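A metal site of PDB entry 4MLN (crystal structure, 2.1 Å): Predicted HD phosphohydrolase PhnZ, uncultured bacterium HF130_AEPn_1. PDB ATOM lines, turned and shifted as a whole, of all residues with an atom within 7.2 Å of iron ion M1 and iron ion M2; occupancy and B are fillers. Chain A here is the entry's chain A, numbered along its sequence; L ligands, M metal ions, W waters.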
ATOM      1  N   GLU A  27       5.730   0.704  -2.792  1.00  0.00           N
ATOM      2  CA  GLU A  27       6.325   2.035  -2.627  1.00  0.00           C
ATOM      3  C   GLU A  27       6.656   2.375  -1.157  1.00  0.00           C
ATOM      4  O   GLU A  27       6.205   1.679  -0.234  1.00  0.00           O
ATOM      5  CB  GLU A  27       5.425   3.097  -3.257  1.00  0.00           C
ATOM      6  CG  GLU A  27       5.063   2.835  -4.718  1.00  0.00           C
ATOM      7  CD  GLU A  27       6.144   3.295  -5.718  1.00  0.00           C
ATOM      8  OE1 GLU A  27       5.800   3.431  -6.922  1.00  0.00           O
ATOM      9  OE2 GLU A  27       7.312   3.521  -5.319  1.00  0.00           O
ATOM     10  N   HIS A  34       1.397   9.556  -1.790  1.00  0.00           N
ATOM     11  CA  HIS A  34       1.949   9.702  -3.129  1.00  0.00           C
ATOM     12  C   HIS A  34       1.162  10.722  -3.972  1.00  0.00           C
ATOM     13  O   HIS A  34       1.732  11.621  -4.577  1.00  0.00           O
ATOM     14  CB  HIS A  34       1.997   8.361  -3.872  1.00  0.00           C
ATOM     15  CG  HIS A  34       2.487   8.474  -5.281  1.00  0.00           C
ATOM     16  ND1 HIS A  34       3.670   9.101  -5.605  1.00  0.00           N
ATOM     17  CD2 HIS A  34       1.945   8.070  -6.459  1.00  0.00           C
ATOM     18  CE1 HIS A  34       3.839   9.066  -6.927  1.00  0.00           C
ATOM     19  NE2 HIS A  34       2.812   8.438  -7.459  1.00  0.00           N
ATOM     20  N   SER A  35      -0.160  10.563  -4.006  1.00  0.00           N
ATOM     21  CA  SER A  35      -1.017  11.508  -4.720  1.00  0.00           C
ATOM     22  C   SER A  35      -0.801  12.945  -4.225  1.00  0.00           C
ATOM     23  O   SER A  35      -0.584  13.858  -5.019  1.00  0.00           O
ATOM     24  CB  SER A  35      -2.490  11.128  -4.574  1.00  0.00           C
ATOM     25  OG  SER A  35      -2.698   9.780  -4.968  1.00  0.00           O
ATOM     26  N   CYS A  38       2.624  14.702  -5.355  1.00  0.00           N
ATOM     27  CA  CYS A  38       2.720  15.124  -6.745  1.00  0.00           C
ATOM     28  C   CYS A  38       1.914  16.397  -6.990  1.00  0.00           C
ATOM     29  O   CYS A  38       2.348  17.290  -7.719  1.00  0.00           O
ATOM     30  CB  CYS A  38       2.243  13.999  -7.675  1.00  0.00           C
ATOM     31  SG  CYS A  38       3.186  12.454  -7.467  1.00  0.00           S
ATOM     32  N   ALA A  55      -1.761  15.630 -11.790  1.00  0.00           N
ATOM     33  CA  ALA A  55      -0.725  15.153 -10.862  1.00  0.00           C
ATOM     34  C   ALA A  55      -1.346  14.494  -9.643  1.00  0.00           C
ATOM     35  O   ALA A  55      -0.920  13.430  -9.215  1.00  0.00           O
ATOM     36  CB  ALA A  55       0.177  16.307 -10.415  1.00  0.00           C
ATOM     37  N   HIS A  58      -3.261  11.084 -10.901  1.00  0.00           N
ATOM     38  CA  HIS A  58      -2.632  10.248 -11.914  1.00  0.00           C
ATOM     39  C   HIS A  58      -2.621   8.753 -11.591  1.00  0.00           C
ATOM     40  O   HIS A  58      -2.649   7.931 -12.505  1.00  0.00           O
ATOM     41  CB  HIS A  58      -1.212  10.738 -12.259  1.00  0.00           C
ATOM     42  CG  HIS A  58      -0.158  10.251 -11.321  1.00  0.00           C
ATOM     43  ND1 HIS A  58       0.191  10.937 -10.172  1.00  0.00           N
ATOM     44  CD2 HIS A  58       0.628   9.151 -11.357  1.00  0.00           C
ATOM     45  CE1 HIS A  58       1.141  10.278  -9.543  1.00  0.00           C
ATOM     46  NE2 HIS A  58       1.430   9.190 -10.242  1.00  0.00           N
ATOM     47  N   ASP A  59      -2.558   8.400 -10.303  1.00  0.00           N
ATOM     48  CA  ASP A  59      -2.583   6.982  -9.904  1.00  0.00           C
ATOM     49  C   ASP A  59      -3.949   6.502  -9.333  1.00  0.00           C
ATOM     50  O   ASP A  59      -4.017   5.459  -8.667  1.00  0.00           O
ATOM     51  CB  ASP A  59      -1.459   6.658  -8.920  1.00  0.00           C
ATOM     52  CG  ASP A  59      -0.134   6.406  -9.604  1.00  0.00           C
ATOM     53  OD1 ASP A  59      -0.116   6.071 -10.817  1.00  0.00           O
ATOM     54  OD2 ASP A  59       0.899   6.522  -8.941  1.00  0.00           O
ATOM     55  N   LEU A  60      -5.003   7.251  -9.626  1.00  0.00           N
ATOM     56  CA  LEU A  60      -6.370   6.884  -9.222  1.00  0.00           C
ATOM     57  C   LEU A  60      -6.739   5.437  -9.609  1.00  0.00           C
ATOM     58  O   LEU A  60      -7.457   4.750  -8.884  1.00  0.00           O
ATOM     59  CB  LEU A  60      -7.370   7.841  -9.868  1.00  0.00           C
ATOM     60  CG  LEU A  60      -8.878   7.718  -9.581  1.00  0.00           C
ATOM     61  CD1 LEU A  60      -9.195   8.034  -8.124  1.00  0.00           C
ATOM     62  CD2 LEU A  60      -9.680   8.638 -10.529  1.00  0.00           C
ATOM     63  N   HIS A  62      -5.241   2.663  -9.690  1.00  0.00           N
ATOM     64  CA  HIS A  62      -4.796   1.585  -8.848  1.00  0.00           C
ATOM     65  C   HIS A  62      -5.938   1.142  -7.905  1.00  0.00           C
ATOM     66  O   HIS A  62      -5.855   0.078  -7.281  1.00  0.00           O
ATOM     67  CB  HIS A  62      -3.562   1.990  -8.035  1.00  0.00           C
ATOM     68  CG  HIS A  62      -2.267   1.968  -8.807  1.00  0.00           C
ATOM     69  ND1 HIS A  62      -1.915   0.945  -9.663  1.00  0.00           N
ATOM     70  CD2 HIS A  62      -1.212   2.824  -8.803  1.00  0.00           C
ATOM     71  CE1 HIS A  62      -0.724   1.184 -10.172  1.00  0.00           C
ATOM     72  NE2 HIS A  62      -0.259   2.314  -9.663  1.00  0.00           N
ATOM     73  N   MET A  72      -0.008  -6.642 -11.603  1.00  0.00           N
ATOM     74  CA  MET A  72       1.369  -6.355 -11.957  1.00  0.00           C
ATOM     75  C   MET A  72       2.263  -6.942 -10.873  1.00  0.00           C
ATOM     76  O   MET A  72       3.149  -6.271 -10.340  1.00  0.00           O
ATOM     77  CB  MET A  72       1.589  -4.849 -12.160  1.00  0.00           C
ATOM     78  CG  MET A  72       0.640  -4.275 -13.207  1.00  0.00           C
ATOM     79  SD  MET A  72       1.171  -2.765 -14.015  1.00  0.00           S
ATOM     80  CE  MET A  72       0.764  -1.540 -12.756  1.00  0.00           C
ATOM     81  N   HIS A  80      -3.652   0.788 -14.957  1.00  0.00           N
ATOM     82  CA  HIS A  80      -4.121   1.803 -14.018  1.00  0.00           C
ATOM     83  C   HIS A  80      -4.212   3.198 -14.656  1.00  0.00           C
ATOM     84  O   HIS A  80      -5.116   3.958 -14.344  1.00  0.00           O
ATOM     85  CB  HIS A  80      -3.275   1.842 -12.739  1.00  0.00           C
ATOM     86  CG  HIS A  80      -1.921   2.486 -12.919  1.00  0.00           C
ATOM     87  ND1 HIS A  80      -0.904   1.898 -13.642  1.00  0.00           N
ATOM     88  CD2 HIS A  80      -1.403   3.639 -12.425  1.00  0.00           C
ATOM     89  CE1 HIS A  80       0.166   2.675 -13.599  1.00  0.00           C
ATOM     90  NE2 HIS A  80      -0.114   3.743 -12.873  1.00  0.00           N
ATOM     91  N   GLU A  81      -3.300   3.537 -15.550  1.00  0.00           N
ATOM     92  CA  GLU A  81      -3.356   4.854 -16.183  1.00  0.00           C
ATOM     93  C   GLU A  81      -4.632   5.007 -17.008  1.00  0.00           C
ATOM     94  O   GLU A  81      -5.270   6.065 -17.004  1.00  0.00           O
ATOM     95  CB  GLU A  81      -2.141   5.069 -17.094  1.00  0.00           C
ATOM     96  CG  GLU A  81      -2.180   4.282 -18.393  1.00  0.00           C
ATOM     97  CD  GLU A  81      -1.630   2.867 -18.255  1.00  0.00           C
ATOM     98  OE1 GLU A  81      -1.444   2.392 -17.132  1.00  0.00           O
ATOM     99  OE2 GLU A  81      -1.365   2.242 -19.293  1.00  0.00           O
ATOM    100  N   ILE A 101      -3.084  11.957 -17.710  1.00  0.00           N
ATOM    101  CA  ILE A 101      -3.083  10.805 -16.813  1.00  0.00           C
ATOM    102  C   ILE A 101      -2.763   9.539 -17.594  1.00  0.00           C
ATOM    103  O   ILE A 101      -1.927   8.737 -17.197  1.00  0.00           O
ATOM    104  CB  ILE A 101      -4.440  10.664 -16.083  1.00  0.00           C
ATOM    105  CG1 ILE A 101      -4.640  11.823 -15.100  1.00  0.00           C
ATOM    106  CG2 ILE A 101      -4.525   9.319 -15.383  1.00  0.00           C
ATOM    107  CD1 ILE A 101      -5.994  11.803 -14.364  1.00  0.00           C
ATOM    108  N   HIS A 104       1.009   9.077 -18.446  1.00  0.00           N
ATOM    109  CA  HIS A 104       2.076   9.051 -17.448  1.00  0.00           C
ATOM    110  C   HIS A 104       2.868   7.751 -17.500  1.00  0.00           C
ATOM    111  O   HIS A 104       4.021   7.717 -17.074  1.00  0.00           O
ATOM    112  CB  HIS A 104       1.578   9.418 -16.023  1.00  0.00           C
ATOM    113  CG  HIS A 104       1.108   8.252 -15.188  1.00  0.00           C
ATOM    114  ND1 HIS A 104      -0.205   7.812 -15.195  1.00  0.00           N
ATOM    115  CD2 HIS A 104       1.757   7.484 -14.286  1.00  0.00           C
ATOM    116  CE1 HIS A 104      -0.326   6.804 -14.339  1.00  0.00           C
ATOM    117  NE2 HIS A 104       0.843   6.588 -13.785  1.00  0.00           N
ATOM    118  N   VAL A 105       2.263   6.695 -18.051  1.00  0.00           N
ATOM    119  CA  VAL A 105       2.974   5.412 -18.183  1.00  0.00           C
ATOM    120  C   VAL A 105       3.812   5.391 -19.445  1.00  0.00           C
ATOM    121  O   VAL A 105       4.980   4.992 -19.419  1.00  0.00           O
ATOM    122  CB  VAL A 105       2.018   4.179 -18.147  1.00  0.00           C
ATOM    123  CG1 VAL A 105       2.759   2.912 -18.595  1.00  0.00           C
ATOM    124  CG2 VAL A 105       1.438   4.012 -16.756  1.00  0.00           C
ATOM    125  N   LYS A 108       6.990   7.073 -18.807  1.00  0.00           N
ATOM    126  CA  LYS A 108       7.978   6.216 -18.187  1.00  0.00           C
ATOM    127  C   LYS A 108       8.665   5.344 -19.238  1.00  0.00           C
ATOM    128  O   LYS A 108       9.884   5.168 -19.218  1.00  0.00           O
ATOM    129  CB  LYS A 108       7.334   5.308 -17.130  1.00  0.00           C
ATOM    130  CG  LYS A 108       8.327   4.738 -16.139  1.00  0.00           C
ATOM    131  CD  LYS A 108       8.062   3.287 -15.741  1.00  0.00           C
ATOM    132  CE  LYS A 108       6.601   2.997 -15.503  1.00  0.00           C
ATOM    133  NZ  LYS A 108       6.418   1.755 -14.680  1.00  0.00           N
ATOM    134  N   SER A 126       8.303   0.824  -9.798  1.00  0.00           N
ATOM    135  CA  SER A 126       8.093   1.320 -11.164  1.00  0.00           C
ATOM    136  C   SER A 126       8.840   0.511 -12.223  1.00  0.00           C
ATOM    137  O   SER A 126       8.283   0.184 -13.280  1.00  0.00           O
ATOM    138  CB  SER A 126       8.426   2.811 -11.280  1.00  0.00           C
ATOM    139  OG  SER A 126       7.405   3.602 -10.688  1.00  0.00           O
ATOM    140  N   THR A 129       6.843  -2.611 -12.837  1.00  0.00           N
ATOM    141  CA  THR A 129       5.572  -2.499 -13.545  1.00  0.00           C
ATOM    142  C   THR A 129       5.787  -2.300 -15.027  1.00  0.00           C
ATOM    143  O   THR A 129       4.941  -2.665 -15.836  1.00  0.00           O
ATOM    144  CB  THR A 129       4.684  -1.371 -12.991  1.00  0.00           C
ATOM    145  OG1 THR A 129       5.395  -0.141 -13.063  1.00  0.00           O
ATOM    146  CG2 THR A 129       4.286  -1.660 -11.547  1.00  0.00           C
ATOM    147  N   GLN A 133       3.592  -3.290 -18.889  1.00  0.00           N
ATOM    148  CA  GLN A 133       3.135  -2.074 -19.559  1.00  0.00           C
ATOM    149  C   GLN A 133       3.631  -1.960 -20.999  1.00  0.00           C
ATOM    150  O   GLN A 133       3.341  -0.986 -21.699  1.00  0.00           O
ATOM    151  CB  GLN A 133       3.531  -0.842 -18.717  1.00  0.00           C
ATOM    152  CG  GLN A 133       2.782  -0.797 -17.391  1.00  0.00           C
ATOM    153  CD  GLN A 133       3.374   0.153 -16.345  1.00  0.00           C
ATOM    154  OE1 GLN A 133       4.550   0.485 -16.352  1.00  0.00           O
ATOM    155  NE2 GLN A 133       2.520   0.567 -15.409  1.00  0.00           N
ATOM    156  N   ARG A 158       5.336  13.121 -15.210  1.00  0.00           N
ATOM    157  CA  ARG A 158       6.134  11.957 -14.838  1.00  0.00           C
ATOM    158  C   ARG A 158       7.244  12.344 -13.867  1.00  0.00           C
ATOM    159  O   ARG A 158       7.572  11.589 -12.928  1.00  0.00           O
ATOM    160  CB  ARG A 158       6.667  11.229 -16.074  1.00  0.00           C
ATOM    161  CG  ARG A 158       7.217   9.853 -15.796  1.00  0.00           C
ATOM    162  CD  ARG A 158       6.134   8.899 -15.359  1.00  0.00           C
ATOM    163  NE  ARG A 158       6.627   7.931 -14.370  1.00  0.00           N
ATOM    164  CZ  ARG A 158       5.976   6.811 -14.028  1.00  0.00           C
ATOM    165  NH1 ARG A 158       4.827   6.508 -14.616  1.00  0.00           N
ATOM    166  NH2 ARG A 158       6.491   6.006 -13.112  1.00  0.00           N
ATOM    167  N   TRP A 160       7.274  14.731 -11.549  1.00  0.00           N
ATOM    168  CA  TRP A 160       6.718  14.856 -10.225  1.00  0.00           C
ATOM    169  C   TRP A 160       6.376  13.499  -9.660  1.00  0.00           C
ATOM    170  O   TRP A 160       6.491  13.260  -8.452  1.00  0.00           O
ATOM    171  CB  TRP A 160       5.473  15.743 -10.276  1.00  0.00           C
ATOM    172  CG  TRP A 160       5.802  17.156 -10.581  1.00  0.00           C
ATOM    173  CD1 TRP A 160       6.854  17.876 -10.101  1.00  0.00           C
ATOM    174  CD2 TRP A 160       5.078  18.040 -11.463  1.00  0.00           C
ATOM    175  NE1 TRP A 160       6.826  19.153 -10.616  1.00  0.00           N
ATOM    176  CE2 TRP A 160       5.749  19.276 -11.444  1.00  0.00           C
ATOM    177  CE3 TRP A 160       3.927  17.898 -12.241  1.00  0.00           C
ATOM    178  CZ2 TRP A 160       5.308  20.364 -12.191  1.00  0.00           C
ATOM    179  CZ3 TRP A 160       3.499  18.966 -12.970  1.00  0.00           C
ATOM    180  CH2 TRP A 160       4.179  20.193 -12.945  1.00  0.00           C
ATOM    181  N   ASP A 161       5.933  12.606 -10.548  1.00  0.00           N
ATOM    182  CA  ASP A 161       5.547  11.259 -10.169  1.00  0.00           C
ATOM    183  C   ASP A 161       6.756  10.593  -9.508  1.00  0.00           C
ATOM    184  O   ASP A 161       6.630  10.033  -8.417  1.00  0.00           O
ATOM    185  CB  ASP A 161       5.097  10.479 -11.415  1.00  0.00           C
ATOM    186  CG  ASP A 161       4.522   9.103 -11.086  1.00  0.00           C
ATOM    187  OD1 ASP A 161       4.226   8.803  -9.920  1.00  0.00           O
ATOM    188  OD2 ASP A 161       4.338   8.313 -12.031  1.00  0.00           O
ATOM    189  N   GLU A 162       7.922  10.672 -10.141  1.00  0.00           N
ATOM    190  CA  GLU A 162       9.107  10.037  -9.562  1.00  0.00           C
ATOM    191  C   GLU A 162       9.559  10.746  -8.272  1.00  0.00           C
ATOM    192  O   GLU A 162      10.220  10.140  -7.425  1.00  0.00           O
ATOM    193  CB  GLU A 162      10.269   9.970 -10.560  1.00  0.00           C
ATOM    194  CG  GLU A 162       9.865   9.826 -12.018  1.00  0.00           C
ATOM    195  CD  GLU A 162       9.291   8.468 -12.379  1.00  0.00           C
ATOM    196  OE1 GLU A 162       9.271   7.536 -11.543  1.00  0.00           O
ATOM    197  OE2 GLU A 162       8.843   8.339 -13.539  1.00  0.00           O
ATOM    198  N   GLY A 164       7.405  12.297  -6.002  1.00  0.00           N
ATOM    199  CA  GLY A 164       6.425  12.093  -4.957  1.00  0.00           C
ATOM    200  C   GLY A 164       6.544  10.817  -4.136  1.00  0.00           C
ATOM    201  O   GLY A 164       5.549  10.082  -3.951  1.00  0.00           O
HETATM  202  O1  LIG L   1       3.643   2.089 -13.000  1.00  0.00           O
HETATM  203  P1  LIG L   1       3.867   3.446 -12.412  1.00  0.00           P
HETATM  204  O2  LIG L   1       3.131   4.360 -13.335  1.00  0.00           O
HETATM  205  O3  LIG L   1       5.327   3.696 -12.606  1.00  0.00           O
HETATM  206  C1  LIG L   1       3.393   3.620 -10.671  1.00  0.00           C
HETATM  207  O4  LIG L   1       2.036   3.848 -10.594  1.00  0.00           O
HETATM  208  C2  LIG L   1       3.808   2.382  -9.945  1.00  0.00           C
HETATM  209  N1  LIG L   1       3.578   2.522  -8.527  1.00  0.00           N
HETATM  210 FE    FE M   1       2.574   7.619  -9.518  1.00  0.00          FE
HETATM  211 FE    FE M   2       1.373   5.275 -12.168  1.00  0.00          FE
HETATM  212  O   HOH W   1       3.794   6.032  -8.762  1.00  0.00           O
HETATM  213  O   HOH W   2       2.669   6.675 -11.381  1.00  0.00           O
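Four residues have an atom within 4 Å of iron ion M1: His 34, His 58, Asp 59 and Asp 161.
NH1 of Arg 158 is in salt-bridge range of OD2 of Asp 161, 3.2 Å away. A ring nitrogen (ND1) of His 58 lies within hydrogen-bond range of the backbone carbonyl oxygen (O) of Ala 55 (2.9 Å). The guanidinium group of Arg 158 lies within hydrogen-bond range of the backbone carbonyl oxygen of His 104, 2.9 Å away. A ring nitrogen (ND1) of His 104 sits at hydrogen-bond distance from the backbone carbonyl oxygen (O) of Ile 101 (2.8 Å). The backbone carbonyl oxygen (O) of His 34 sits at hydrogen-bond distance from the side-chain sulfur (SG) of Cys 38 (3.3 Å). ND1 of His 34 lies within hydrogen-bond range of O of Gly 164, 2.7 Å away.
A ring nitrogen (NE2) of His 62 lies close to an oxygen (O4) of the ligand (2.9 Å). The guanidinium group (NH2) of Arg 158 lies within salt-bridge range of an oxygen (O3) of the ligand. O1 of the ligand lies within hydrogen-bond range of NE2 of Gln 133 (3.1 Å). A nitrogen (N1) of the ligand lies within salt-bridge range of the side-chain carboxylate (OE1) of Glu 27, at 2.9 Å. The side-chain hydroxyl of Ser 126 sits at hydrogen-bond distance from an oxygen (O3) of the ligand. An oxygen (O3) of the ligand lies within salt-bridge range of the side-chain amino group (NZ) of Lys 108. The side-chain hydroxyl (OG1) of Thr 129 lies within hydrogen-bond range of an oxygen (O1) of the ligand (2.8 Å).
Iron ion M1 is bound by OD1 of Asp 161 (2.1 Å), NE2 of His 58 (2.1 Å), OD2 of Asp 59 (2.1 Å), water W2 (2.1 Å), water W1 (2.1 Å) and NE2 of His 34 (2.2 Å). Iron ion M1 has six donor atoms within binding distance.
Water W2 is bound to iron ion M2 (2.1 Å). NE2 of His 104 is bound to iron ion M2. The side-chain carboxylate (OD1) of Asp 59 binds iron ion M2 (2.2 Å). Iron ion M2 is bound by O4 of the ligand (2.2 Å). NE2 of His 80 is bound to iron ion M2, at 2.2 Å. O2 of the ligand is bound to iron ion M2 (2.3 Å).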
